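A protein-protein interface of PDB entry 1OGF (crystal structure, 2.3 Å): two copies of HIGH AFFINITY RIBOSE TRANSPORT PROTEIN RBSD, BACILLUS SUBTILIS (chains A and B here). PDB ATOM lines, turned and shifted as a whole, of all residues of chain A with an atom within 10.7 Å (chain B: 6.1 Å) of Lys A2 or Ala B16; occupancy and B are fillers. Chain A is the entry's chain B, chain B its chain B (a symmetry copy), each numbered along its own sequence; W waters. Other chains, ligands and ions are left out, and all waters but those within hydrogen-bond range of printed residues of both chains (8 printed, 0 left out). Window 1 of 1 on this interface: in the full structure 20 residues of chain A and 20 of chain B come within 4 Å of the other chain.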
ATOM      1  N   MET A   1      17.537   4.464 -24.711  1.00  0.00           N
ATOM      2  CA  MET A   1      18.034   3.178 -24.140  1.00  0.00           C
ATOM      3  C   MET A   1      17.430   2.898 -22.776  1.00  0.00           C
ATOM      4  O   MET A   1      17.017   3.817 -22.062  1.00  0.00           O
ATOM      5  CB  MET A   1      19.562   3.197 -24.005  1.00  0.00           C
ATOM      6  CG  MET A   1      20.321   3.045 -25.316  1.00  0.00           C
ATOM      7  SD  MET A   1      22.118   2.939 -25.074  1.00  0.00           S
ATOM      8  CE  MET A   1      22.230   1.441 -24.106  1.00  0.00           C
ATOM      9  N   LYS A   2      17.386   1.618 -22.426  1.00  0.00           N
ATOM     10  CA  LYS A   2      16.853   1.175 -21.144  1.00  0.00           C
ATOM     11  C   LYS A   2      17.849   1.627 -20.063  1.00  0.00           C
ATOM     12  O   LYS A   2      19.045   1.364 -20.169  1.00  0.00           O
ATOM     13  CB  LYS A   2      16.703  -0.357 -21.162  1.00  0.00           C
ATOM     14  CG  LYS A   2      16.050  -0.965 -19.920  1.00  0.00           C
ATOM     15  CD  LYS A   2      15.643  -2.425 -20.150  1.00  0.00           C
ATOM     16  CE  LYS A   2      16.837  -3.355 -20.314  1.00  0.00           C
ATOM     17  NZ  LYS A   2      17.459  -3.697 -19.000  1.00  0.00           N
ATOM     18  N   LYS A   3      17.358   2.308 -19.033  1.00  0.00           N
ATOM     19  CA  LYS A   3      18.232   2.817 -17.971  1.00  0.00           C
ATOM     20  C   LYS A   3      18.722   1.787 -16.962  1.00  0.00           C
ATOM     21  O   LYS A   3      19.883   1.810 -16.552  1.00  0.00           O
ATOM     22  CB  LYS A   3      17.531   3.924 -17.178  1.00  0.00           C
ATOM     23  CG  LYS A   3      17.530   5.301 -17.798  1.00  0.00           C
ATOM     24  CD  LYS A   3      16.918   6.272 -16.799  1.00  0.00           C
ATOM     25  CE  LYS A   3      16.824   7.679 -17.340  1.00  0.00           C
ATOM     26  NZ  LYS A   3      16.028   8.532 -16.421  1.00  0.00           N
ATOM     27  N   HIS A   4      17.837   0.884 -16.561  1.00  0.00           N
ATOM     28  CA  HIS A   4      18.183  -0.089 -15.547  1.00  0.00           C
ATOM     29  C   HIS A   4      18.033  -1.550 -15.946  1.00  0.00           C
ATOM     30  O   HIS A   4      17.382  -1.882 -16.944  1.00  0.00           O
ATOM     31  CB  HIS A   4      17.327   0.196 -14.315  1.00  0.00           C
ATOM     32  CG  HIS A   4      17.316   1.640 -13.918  1.00  0.00           C
ATOM     33  ND1 HIS A   4      16.165   2.314 -13.575  1.00  0.00           N
ATOM     34  CD2 HIS A   4      18.322   2.550 -13.829  1.00  0.00           C
ATOM     35  CE1 HIS A   4      16.457   3.574 -13.296  1.00  0.00           C
ATOM     36  NE2 HIS A   4      17.761   3.738 -13.444  1.00  0.00           N
ATOM     37  N   GLY A   5      18.656  -2.419 -15.155  1.00  0.00           N
ATOM     38  CA  GLY A   5      18.555  -3.846 -15.390  1.00  0.00           C
ATOM     39  C   GLY A   5      19.621  -4.453 -16.268  1.00  0.00           C
ATOM     40  O   GLY A   5      20.528  -3.773 -16.739  1.00  0.00           O
ATOM     41  N   ILE A   6      19.499  -5.756 -16.487  1.00  0.00           N
ATOM     42  CA  ILE A   6      20.451  -6.487 -17.297  1.00  0.00           C
ATOM     43  C   ILE A   6      20.575  -5.828 -18.681  1.00  0.00           C
ATOM     44  O   ILE A   6      19.597  -5.307 -19.237  1.00  0.00           O
ATOM     45  CB  ILE A   6      20.010  -7.953 -17.397  1.00  0.00           C
ATOM     46  CG1 ILE A   6      21.205  -8.830 -17.768  1.00  0.00           C
ATOM     47  CG2 ILE A   6      18.840  -8.085 -18.381  1.00  0.00           C
ATOM     48  CD1 ILE A   6      20.984 -10.303 -17.468  1.00  0.00           C
ATOM     49  N   LEU A   7      21.793  -5.828 -19.216  1.00  0.00           N
ATOM     50  CA  LEU A   7      22.078  -5.203 -20.502  1.00  0.00           C
ATOM     51  C   LEU A   7      21.589  -5.983 -21.716  1.00  0.00           C
ATOM     52  O   LEU A   7      21.093  -5.390 -22.672  1.00  0.00           O
ATOM     53  CB  LEU A   7      23.588  -4.954 -20.634  1.00  0.00           C
ATOM     54  CG  LEU A   7      24.086  -4.289 -21.917  1.00  0.00           C
ATOM     55  CD1 LEU A   7      23.367  -2.963 -22.139  1.00  0.00           C
ATOM     56  CD2 LEU A   7      25.597  -4.083 -21.831  1.00  0.00           C
ATOM     57  N   ASN A   8      21.741  -7.301 -21.684  1.00  0.00           N
ATOM     58  CA  ASN A   8      21.324  -8.128 -22.808  1.00  0.00           C
ATOM     59  C   ASN A   8      19.814  -8.048 -23.039  1.00  0.00           C
ATOM     60  O   ASN A   8      19.024  -8.347 -22.144  1.00  0.00           O
ATOM     61  CB  ASN A   8      21.751  -9.583 -22.582  1.00  0.00           C
ATOM     62  CG  ASN A   8      21.602 -10.430 -23.826  1.00  0.00           C
ATOM     63  OD1 ASN A   8      20.496 -10.825 -24.192  1.00  0.00           O
ATOM     64  ND2 ASN A   8      22.717 -10.697 -24.499  1.00  0.00           N
ATOM     65  N   SER A   9      19.428  -7.636 -24.245  1.00  0.00           N
ATOM     66  CA  SER A   9      18.019  -7.506 -24.608  1.00  0.00           C
ATOM     67  C   SER A   9      17.293  -8.842 -24.524  1.00  0.00           C
ATOM     68  O   SER A   9      16.190  -8.911 -23.975  1.00  0.00           O
ATOM     69  CB  SER A   9      17.877  -6.936 -26.029  1.00  0.00           C
ATOM     70  OG  SER A   9      18.501  -7.775 -26.989  1.00  0.00           O
ATOM     71  N   HIS A  10      17.900  -9.898 -25.069  1.00  0.00           N
ATOM     72  CA  HIS A  10      17.279 -11.225 -25.029  1.00  0.00           C
ATOM     73  C   HIS A  10      17.035 -11.636 -23.579  1.00  0.00           C
ATOM     74  O   HIS A  10      15.961 -12.145 -23.250  1.00  0.00           O
ATOM     75  CB  HIS A  10      18.165 -12.285 -25.701  1.00  0.00           C
ATOM     76  CG  HIS A  10      18.538 -11.966 -27.122  1.00  0.00           C
ATOM     77  ND1 HIS A  10      17.601 -11.680 -28.095  1.00  0.00           N
ATOM     78  CD2 HIS A  10      19.746 -11.871 -27.722  1.00  0.00           C
ATOM     79  CE1 HIS A  10      18.221 -11.419 -29.233  1.00  0.00           C
ATOM     80  NE2 HIS A  10      19.522 -11.525 -29.037  1.00  0.00           N
ATOM     81  N   LEU A  11      18.032 -11.409 -22.717  1.00  0.00           N
ATOM     82  CA  LEU A  11      17.933 -11.764 -21.301  1.00  0.00           C
ATOM     83  C   LEU A  11      16.909 -10.936 -20.542  1.00  0.00           C
ATOM     84  O   LEU A  11      16.216 -11.447 -19.664  1.00  0.00           O
ATOM     85  CB  LEU A  11      19.302 -11.643 -20.611  1.00  0.00           C
ATOM     86  CG  LEU A  11      20.353 -12.699 -20.988  1.00  0.00           C
ATOM     87  CD1 LEU A  11      21.584 -12.587 -20.078  1.00  0.00           C
ATOM     88  CD2 LEU A  11      19.735 -14.079 -20.850  1.00  0.00           C
ATOM     89  N   ALA A  12      16.823  -9.655 -20.872  1.00  0.00           N
ATOM     90  CA  ALA A  12      15.861  -8.768 -20.225  1.00  0.00           C
ATOM     91  C   ALA A  12      14.436  -9.289 -20.479  1.00  0.00           C
ATOM     92  O   ALA A  12      13.584  -9.279 -19.589  1.00  0.00           O
ATOM     93  CB  ALA A  12      16.013  -7.352 -20.774  1.00  0.00           C
ATOM     94  N   LYS A  13      14.183  -9.754 -21.697  1.00  0.00           N
ATOM     95  CA  LYS A  13      12.862 -10.269 -22.043  1.00  0.00           C
ATOM     96  C   LYS A  13      12.515 -11.488 -21.207  1.00  0.00           C
ATOM     97  O   LYS A  13      11.379 -11.635 -20.765  1.00  0.00           O
ATOM     98  CB  LYS A  13      12.804 -10.610 -23.535  1.00  0.00           C
ATOM     99  CG  LYS A  13      12.914  -9.386 -24.430  1.00  0.00           C
ATOM    100  CD  LYS A  13      13.024  -9.758 -25.898  1.00  0.00           C
ATOM    101  CE  LYS A  13      13.159  -8.506 -26.756  1.00  0.00           C
ATOM    102  NZ  LYS A  13      13.360  -8.844 -28.189  1.00  0.00           N
ATOM    103  N   ILE A  14      13.499 -12.355 -20.980  1.00  0.00           N
ATOM    104  CA  ILE A  14      13.290 -13.559 -20.181  1.00  0.00           C
ATOM    105  C   ILE A  14      13.005 -13.221 -18.724  1.00  0.00           C
ATOM    106  O   ILE A  14      12.101 -13.787 -18.116  1.00  0.00           O
ATOM    107  CB  ILE A  14      14.526 -14.494 -20.219  1.00  0.00           C
ATOM    108  CG1 ILE A  14      14.813 -14.948 -21.653  1.00  0.00           C
ATOM    109  CG2 ILE A  14      14.287 -15.699 -19.322  1.00  0.00           C
ATOM    110  CD1 ILE A  14      13.660 -15.658 -22.317  1.00  0.00           C
ATOM    111  N   LEU A  15      13.783 -12.307 -18.150  1.00  0.00           N
ATOM    112  CA  LEU A  15      13.575 -11.932 -16.754  1.00  0.00           C
ATOM    113  C   LEU A  15      12.233 -11.239 -16.568  1.00  0.00           C
ATOM    114  O   LEU A  15      11.504 -11.507 -15.601  1.00  0.00           O
ATOM    115  CB  LEU A  15      14.696 -11.006 -16.263  1.00  0.00           C
ATOM    116  CG  LEU A  15      16.100 -11.613 -16.246  1.00  0.00           C
ATOM    117  CD1 LEU A  15      17.088 -10.641 -15.611  1.00  0.00           C
ATOM    118  CD2 LEU A  15      16.070 -12.914 -15.466  1.00  0.00           C
ATOM    119  N   ALA A  16      11.912 -10.349 -17.496  1.00  0.00           N
ATOM    120  CA  ALA A  16      10.664  -9.606 -17.418  1.00  0.00           C
ATOM    121  C   ALA A  16       9.450 -10.501 -17.187  1.00  0.00           C
ATOM    122  O   ALA A  16       8.516 -10.100 -16.486  1.00  0.00           O
ATOM    123  CB  ALA A  16      10.473  -8.776 -18.677  1.00  0.00           C
ATOM    124  N   ASP A  17       9.459 -11.708 -17.762  1.00  0.00           N
ATOM    125  CA  ASP A  17       8.331 -12.633 -17.605  1.00  0.00           C
ATOM    126  C   ASP A  17       8.445 -13.575 -16.413  1.00  0.00           C
ATOM    127  O   ASP A  17       7.520 -14.337 -16.135  1.00  0.00           O
ATOM    128  CB  ASP A  17       8.126 -13.479 -18.871  1.00  0.00           C
ATOM    129  CG  ASP A  17       7.367 -12.736 -19.952  1.00  0.00           C
ATOM    130  OD1 ASP A  17       6.503 -11.903 -19.596  1.00  0.00           O
ATOM    131  OD2 ASP A  17       7.624 -12.990 -21.150  1.00  0.00           O
ATOM    132  N   ILE A  40      19.512 -18.819 -25.696  1.00  0.00           N
ATOM    133  CA  ILE A  40      20.110 -17.495 -25.840  1.00  0.00           C
ATOM    134  C   ILE A  40      21.617 -17.708 -25.691  1.00  0.00           C
ATOM    135  O   ILE A  40      22.132 -17.810 -24.577  1.00  0.00           O
ATOM    136  CB  ILE A  40      19.616 -16.524 -24.739  1.00  0.00           C
ATOM    137  CG1 ILE A  40      18.091 -16.410 -24.793  1.00  0.00           C
ATOM    138  CG2 ILE A  40      20.245 -15.154 -24.934  1.00  0.00           C
ATOM    139  CD1 ILE A  40      17.491 -15.529 -23.717  1.00  0.00           C
ATOM    140  N   VAL A  57      26.180 -11.943 -13.207  1.00  0.00           N
ATOM    141  CA  VAL A  57      25.255 -10.971 -13.772  1.00  0.00           C
ATOM    142  C   VAL A  57      23.810 -11.357 -13.454  1.00  0.00           C
ATOM    143  O   VAL A  57      23.053 -10.544 -12.922  1.00  0.00           O
ATOM    144  CB  VAL A  57      25.449 -10.850 -15.293  1.00  0.00           C
ATOM    145  CG1 VAL A  57      24.317 -10.038 -15.914  1.00  0.00           C
ATOM    146  CG2 VAL A  57      26.782 -10.166 -15.570  1.00  0.00           C
ATOM    147  N   GLU A  60      22.671 -10.870  -9.884  1.00  0.00           N
ATOM    148  CA  GLU A  60      22.462  -9.483  -9.497  1.00  0.00           C
ATOM    149  C   GLU A  60      21.223  -8.861 -10.133  1.00  0.00           C
ATOM    150  O   GLU A  60      20.740  -7.825  -9.670  1.00  0.00           O
ATOM    151  CB  GLU A  60      23.706  -8.663  -9.853  1.00  0.00           C
ATOM    152  CG  GLU A  60      24.004  -7.530  -8.876  1.00  0.00           C
ATOM    153  CD  GLU A  60      23.270  -6.265  -9.228  1.00  0.00           C
ATOM    154  OE1 GLU A  60      22.599  -5.686  -8.347  1.00  0.00           O
ATOM    155  OE2 GLU A  60      23.374  -5.848 -10.402  1.00  0.00           O
ATOM    156  N   GLU A  61      20.697  -9.495 -11.177  1.00  0.00           N
ATOM    157  CA  GLU A  61      19.513  -8.969 -11.863  1.00  0.00           C
ATOM    158  C   GLU A  61      18.240  -9.802 -11.690  1.00  0.00           C
ATOM    159  O   GLU A  61      17.154  -9.380 -12.092  1.00  0.00           O
ATOM    160  CB  GLU A  61      19.814  -8.816 -13.355  1.00  0.00           C
ATOM    161  CG  GLU A  61      20.985  -7.901 -13.651  1.00  0.00           C
ATOM    162  CD  GLU A  61      20.687  -6.440 -13.358  1.00  0.00           C
ATOM    163  OE1 GLU A  61      19.620  -6.133 -12.784  1.00  0.00           O
ATOM    164  OE2 GLU A  61      21.536  -5.593 -13.702  1.00  0.00           O
ATOM    165  N   LEU B  11       6.433  -3.878 -21.356  1.00  0.00           N
ATOM    166  CA  LEU B  11       7.243  -2.664 -21.467  1.00  0.00           C
ATOM    167  C   LEU B  11       8.736  -2.925 -21.363  1.00  0.00           C
ATOM    168  O   LEU B  11       9.533  -2.288 -22.050  1.00  0.00           O
ATOM    169  CB  LEU B  11       6.827  -1.633 -20.405  1.00  0.00           C
ATOM    170  CG  LEU B  11       5.462  -0.957 -20.605  1.00  0.00           C
ATOM    171  CD1 LEU B  11       5.272   0.189 -19.602  1.00  0.00           C
ATOM    172  CD2 LEU B  11       5.383  -0.419 -22.022  1.00  0.00           C
ATOM    173  N   ALA B  12       9.115  -3.851 -20.493  1.00  0.00           N
ATOM    174  CA  ALA B  12      10.522  -4.200 -20.323  1.00  0.00           C
ATOM    175  C   ALA B  12      11.083  -4.724 -21.656  1.00  0.00           C
ATOM    176  O   ALA B  12      12.208  -4.404 -22.046  1.00  0.00           O
ATOM    177  CB  ALA B  12      10.663  -5.263 -19.236  1.00  0.00           C
ATOM    178  N   LYS B  13      10.290  -5.523 -22.361  1.00  0.00           N
ATOM    179  CA  LYS B  13      10.727  -6.076 -23.639  1.00  0.00           C
ATOM    180  C   LYS B  13      10.977  -4.974 -24.654  1.00  0.00           C
ATOM    181  O   LYS B  13      11.941  -5.036 -25.411  1.00  0.00           O
ATOM    182  CB  LYS B  13       9.684  -7.065 -24.168  1.00  0.00           C
ATOM    183  CG  LYS B  13       9.556  -8.312 -23.308  1.00  0.00           C
ATOM    184  CD  LYS B  13       8.405  -9.198 -23.753  1.00  0.00           C
ATOM    185  CE  LYS B  13       8.294 -10.419 -22.849  1.00  0.00           C
ATOM    186  NZ  LYS B  13       7.120 -11.258 -23.204  1.00  0.00           N
ATOM    187  N   ILE B  14      10.114  -3.962 -24.658  1.00  0.00           N
ATOM    188  CA  ILE B  14      10.256  -2.838 -25.580  1.00  0.00           C
ATOM    189  C   ILE B  14      11.501  -2.016 -25.275  1.00  0.00           C
ATOM    190  O   ILE B  14      12.243  -1.646 -26.179  1.00  0.00           O
ATOM    191  CB  ILE B  14       9.033  -1.888 -25.520  1.00  0.00           C
ATOM    192  CG1 ILE B  14       7.752  -2.633 -25.909  1.00  0.00           C
ATOM    193  CG2 ILE B  14       9.255  -0.703 -26.447  1.00  0.00           C
ATOM    194  CD1 ILE B  14       7.798  -3.261 -27.279  1.00  0.00           C
ATOM    195  N   LEU B  15      11.729  -1.714 -23.999  1.00  0.00           N
ATOM    196  CA  LEU B  15      12.900  -0.926 -23.626  1.00  0.00           C
ATOM    197  C   LEU B  15      14.186  -1.686 -23.914  1.00  0.00           C
ATOM    198  O   LEU B  15      15.164  -1.118 -24.426  1.00  0.00           O
ATOM    199  CB  LEU B  15      12.857  -0.550 -22.138  1.00  0.00           C
ATOM    200  CG  LEU B  15      11.693   0.348 -21.713  1.00  0.00           C
ATOM    201  CD1 LEU B  15      11.846   0.754 -20.252  1.00  0.00           C
ATOM    202  CD2 LEU B  15      11.665   1.578 -22.600  1.00  0.00           C
ATOM    203  N   ALA B  16      14.182  -2.970 -23.585  1.00  0.00           N
ATOM    204  CA  ALA B  16      15.359  -3.798 -23.793  1.00  0.00           C
ATOM    205  C   ALA B  16      15.932  -3.678 -25.202  1.00  0.00           C
ATOM    206  O   ALA B  16      17.152  -3.732 -25.375  1.00  0.00           O
ATOM    207  CB  ALA B  16      15.035  -5.251 -23.479  1.00  0.00           C
ATOM    208  N   ASP B  17      15.063  -3.509 -26.205  1.00  0.00           N
ATOM    209  CA  ASP B  17      15.520  -3.395 -27.595  1.00  0.00           C
ATOM    210  C   ASP B  17      15.806  -1.970 -28.052  1.00  0.00           C
ATOM    211  O   ASP B  17      16.273  -1.761 -29.171  1.00  0.00           O
ATOM    212  CB  ASP B  17      14.508  -4.020 -28.565  1.00  0.00           C
ATOM    213  CG  ASP B  17      14.633  -5.528 -28.648  1.00  0.00           C
ATOM    214  OD1 ASP B  17      15.771  -6.031 -28.502  1.00  0.00           O
ATOM    215  OD2 ASP B  17      13.605  -6.207 -28.867  1.00  0.00           O
ATOM    216  N   LEU B  18      15.526  -0.994 -27.195  1.00  0.00           N
ATOM    217  CA  LEU B  18      15.759   0.402 -27.544  1.00  0.00           C
ATOM    218  C   LEU B  18      17.192   0.719 -27.927  1.00  0.00           C
ATOM    219  O   LEU B  18      18.133   0.429 -27.188  1.00  0.00           O
ATOM    220  CB  LEU B  18      15.352   1.333 -26.395  1.00  0.00           C
ATOM    221  CG  LEU B  18      13.856   1.518 -26.152  1.00  0.00           C
ATOM    222  CD1 LEU B  18      13.635   2.574 -25.089  1.00  0.00           C
ATOM    223  CD2 LEU B  18      13.186   1.926 -27.456  1.00  0.00           C
ATOM    224  N   GLU B  61      12.741   5.050 -16.413  1.00  0.00           N
ATOM    225  CA  GLU B  61      13.304   3.774 -16.865  1.00  0.00           C
ATOM    226  C   GLU B  61      13.905   3.796 -18.274  1.00  0.00           C
ATOM    227  O   GLU B  61      14.540   2.829 -18.699  1.00  0.00           O
ATOM    228  CB  GLU B  61      12.230   2.688 -16.794  1.00  0.00           C
ATOM    229  CG  GLU B  61      11.654   2.490 -15.406  1.00  0.00           C
ATOM    230  CD  GLU B  61      12.638   1.860 -14.436  1.00  0.00           C
ATOM    231  OE1 GLU B  61      13.829   1.701 -14.785  1.00  0.00           O
ATOM    232  OE2 GLU B  61      12.215   1.527 -13.311  1.00  0.00           O
ATOM    233  N   MET B  62      13.711   4.904 -18.982  1.00  0.00           N
ATOM    234  CA  MET B  62      14.204   5.065 -20.347  1.00  0.00           C
ATOM    235  C   MET B  62      15.001   6.355 -20.487  1.00  0.00           C
ATOM    236  O   MET B  62      14.563   7.408 -20.028  1.00  0.00           O
ATOM    237  CB  MET B  62      13.015   5.118 -21.310  1.00  0.00           C
ATOM    238  CG  MET B  62      13.375   5.299 -22.774  1.00  0.00           C
ATOM    239  SD  MET B  62      11.918   5.698 -23.762  1.00  0.00           S
ATOM    240  CE  MET B  62      12.703   6.269 -25.248  1.00  0.00           C
ATOM    241  N   ALA B  63      16.170   6.283 -21.118  1.00  0.00           N
ATOM    242  CA  ALA B  63      16.977   7.482 -21.329  1.00  0.00           C
ATOM    243  C   ALA B  63      16.366   8.209 -22.527  1.00  0.00           C
ATOM    244  O   ALA B  63      16.430   7.717 -23.654  1.00  0.00           O
ATOM    245  CB  ALA B  63      18.420   7.102 -21.622  1.00  0.00           C
ATOM    246  N   LEU B 130      23.446   5.871 -23.368  1.00  0.00           N
ATOM    247  CA  LEU B 130      24.069   5.887 -22.047  1.00  0.00           C
ATOM    248  C   LEU B 130      25.575   6.160 -22.111  1.00  0.00           C
ATOM    249  O   LEU B 130      26.258   6.156 -21.087  1.00  0.00           O
ATOM    250  CB  LEU B 130      23.807   4.554 -21.335  1.00  0.00           C
ATOM    251  CG  LEU B 130      22.339   4.148 -21.161  1.00  0.00           C
ATOM    252  CD1 LEU B 130      22.258   2.772 -20.512  1.00  0.00           C
ATOM    253  CD2 LEU B 130      21.610   5.183 -20.314  1.00  0.00           C
HETATM  254  O   HOH W   1      12.524  -8.169 -31.368  1.00  0.00           O
HETATM  255  O   HOH W   2      16.435  -8.532 -28.601  1.00  0.00           O
HETATM  256  O   HOH W   3      18.652  -4.401 -23.099  1.00  0.00           O
HETATM  257  O   HOH W   4      15.045   0.870 -16.915  1.00  0.00           O
HETATM  258  O   HOH W   5      18.237  -0.181 -24.491  1.00  0.00           O
HETATM  259  O   HOH W   6       4.968 -10.453 -21.096  1.00  0.00           O
HETATM  260  O   HOH W   7      14.084   1.587 -11.369  1.00  0.00           O
HETATM  261  O   HOH W   8       5.947 -14.360 -23.716  1.00  0.00           O
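Of the 21 printed residues of chain A, 9 touch a printed residue of chain B. Hydrophobic or aromatic side chains of chain A that line the printed part of chain B: Met A1, His A4, Ala A12 and Ala A16. Along chain A the printed residues that touch a printed residue of chain B span positions 1 to 17. Printed residues of chain B that touch a printed residue of chain A: Ala B12, Lys B13, Leu B15, Ala B16, Asp B17, Leu B18, Glu B61, Met B62, Ala B63 and Leu B130. Hydrophobic or aromatic side chains of chain B within 4 Å of the printed part of chain A: Ala B12, Leu B15, Ala B16, Leu B18, Met B62, Ala B63 and Leu B130. Among the printed residues, 19 pairs touch across the chains. Among the printed residues, Asp or Glu carboxylates within 4 Å of a Lys or Arg side-chain nitrogen of the other chain: Lys A13 with Asp B17 (2.7 Å) and Asp A17 with Lys B13 (2.7 Å).
N of Ala B63 sits at hydrogen-bond distance from O of Met A1, 2.8 Å away. The side-chain sulfur (SD) of Met A1 sits at hydrogen-bond distance from the backbone NH (N) of Leu B130. The backbone NH (N) of Lys A3 is in hydrogen-bond range of the backbone carbonyl oxygen (O) of Glu B61, at 2.9 Å. The side-chain carboxylate of Glu B61 is in hydrogen-bond range of a ring nitrogen (ND1) of His A4. NZ of Lys A13 is in salt-bridge range of OD2 of Asp B17 (2.7 Å). The side-chain carboxylate of Asp A17 is in salt-bridge range of the side-chain amino group of Lys B13 (2.7 Å).
The side-chain amino group (NZ) of Lys A2 sits at hydrogen-bond distance from the backbone carbonyl oxygen (O) of His A4 (2.7 Å). NZ of Lys A2 sits at hydrogen-bond distance from O of Ile A6 (2.7 Å).
Leu B18 touches Met A1 (O to CG, 3.9 Å). Met A1 touches Met B62 (O to CA, 3.5 Å). Ala B16 touches Lys A2 (N to CD, 3.8 Å). Leu B130 touches Lys A2. Lys A3 touches Met B62. Ala B63 touches Lys A3. Ser A9 touches Ala B16. Ala A12 touches Ala B16 (CB to CB, 3.6 Å). CG of Lys A13 touches CG of Lys B13, at 3.7 Å. Ala A16 touches Ala B12 (CB to CB, 3.6 Å).
Water W4 lies within hydrogen-bond range of the side-chain carboxylate of Glu B61 (2.6 Å), the backbone NH of His A4 (2.8 Å) and the backbone NH of Lys A3 (3.5 Å). Water W2 lies within hydrogen-bond range of the side-chain carboxylate of Asp B17 (2.6 Å), the side-chain hydroxyl of Ser A9 (2.7 Å), the side-chain amino group of Lys A13 (3.1 Å) and a ring nitrogen (ND1) of His A10 (3.4 Å). Water W3 lies within hydrogen-bond range of the backbone carbonyl oxygen of Leu A7 and the backbone carbonyl oxygen of Ala B16. Water W5 lies within hydrogen-bond range of the backbone carbonyl oxygen (O) of Leu B18, the backbone NH (N) of Lys A2 and the backbone carbonyl oxygen (O) of Leu B15. Water W8 bridges the side-chain amino group (NZ) of Lys B13 and the side-chain carboxylate (OD2) of Asp A17. Water W1 bridges the side-chain amino group (NZ) of Lys A13 (3.4 Å) and the side-chain carboxylate (OD2) of Asp B17 (3.4 Å).
Lys A2 touches four residues of chain B. Ala B16 touches three residues of chain A. Printed residues of chain A within 4 Å of Leu B15: Lys A2. Of chain A, only Ser A9 and Lys A13 come within 4 Å of Asp B17. Of chain A, only Met A1 comes within 4 Å of Leu B18. Of the printed residues of chain B, Ala A12 touches Ala B16. Of the printed residues of chain B, Met A1 touches Leu B18, Met B62, Ala B63 and Leu B130. Of the printed residues of chain B, Asp A17 touches Lys B13. Ile A40 touches none of the printed residues of chain B. The nearest residue of chain B that does not touch Lys A2 is Ala B12 (4.4 Å). The nearest residue of chain A that does not touch Ala B16 is Lys A13 (4.7 Å). The nearest printed residue of chain B that does not touch Ala A16 is Lys B13 (4.7 Å).
Ala A12 touches Ala B16, and with the chains exchanged Ala A16 touches Ala B12. Lys A13 touches its own counterpart, Lys B13. Lys A13 touches Asp B17, and with the chains exchanged Asp A17 touches Lys B13.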
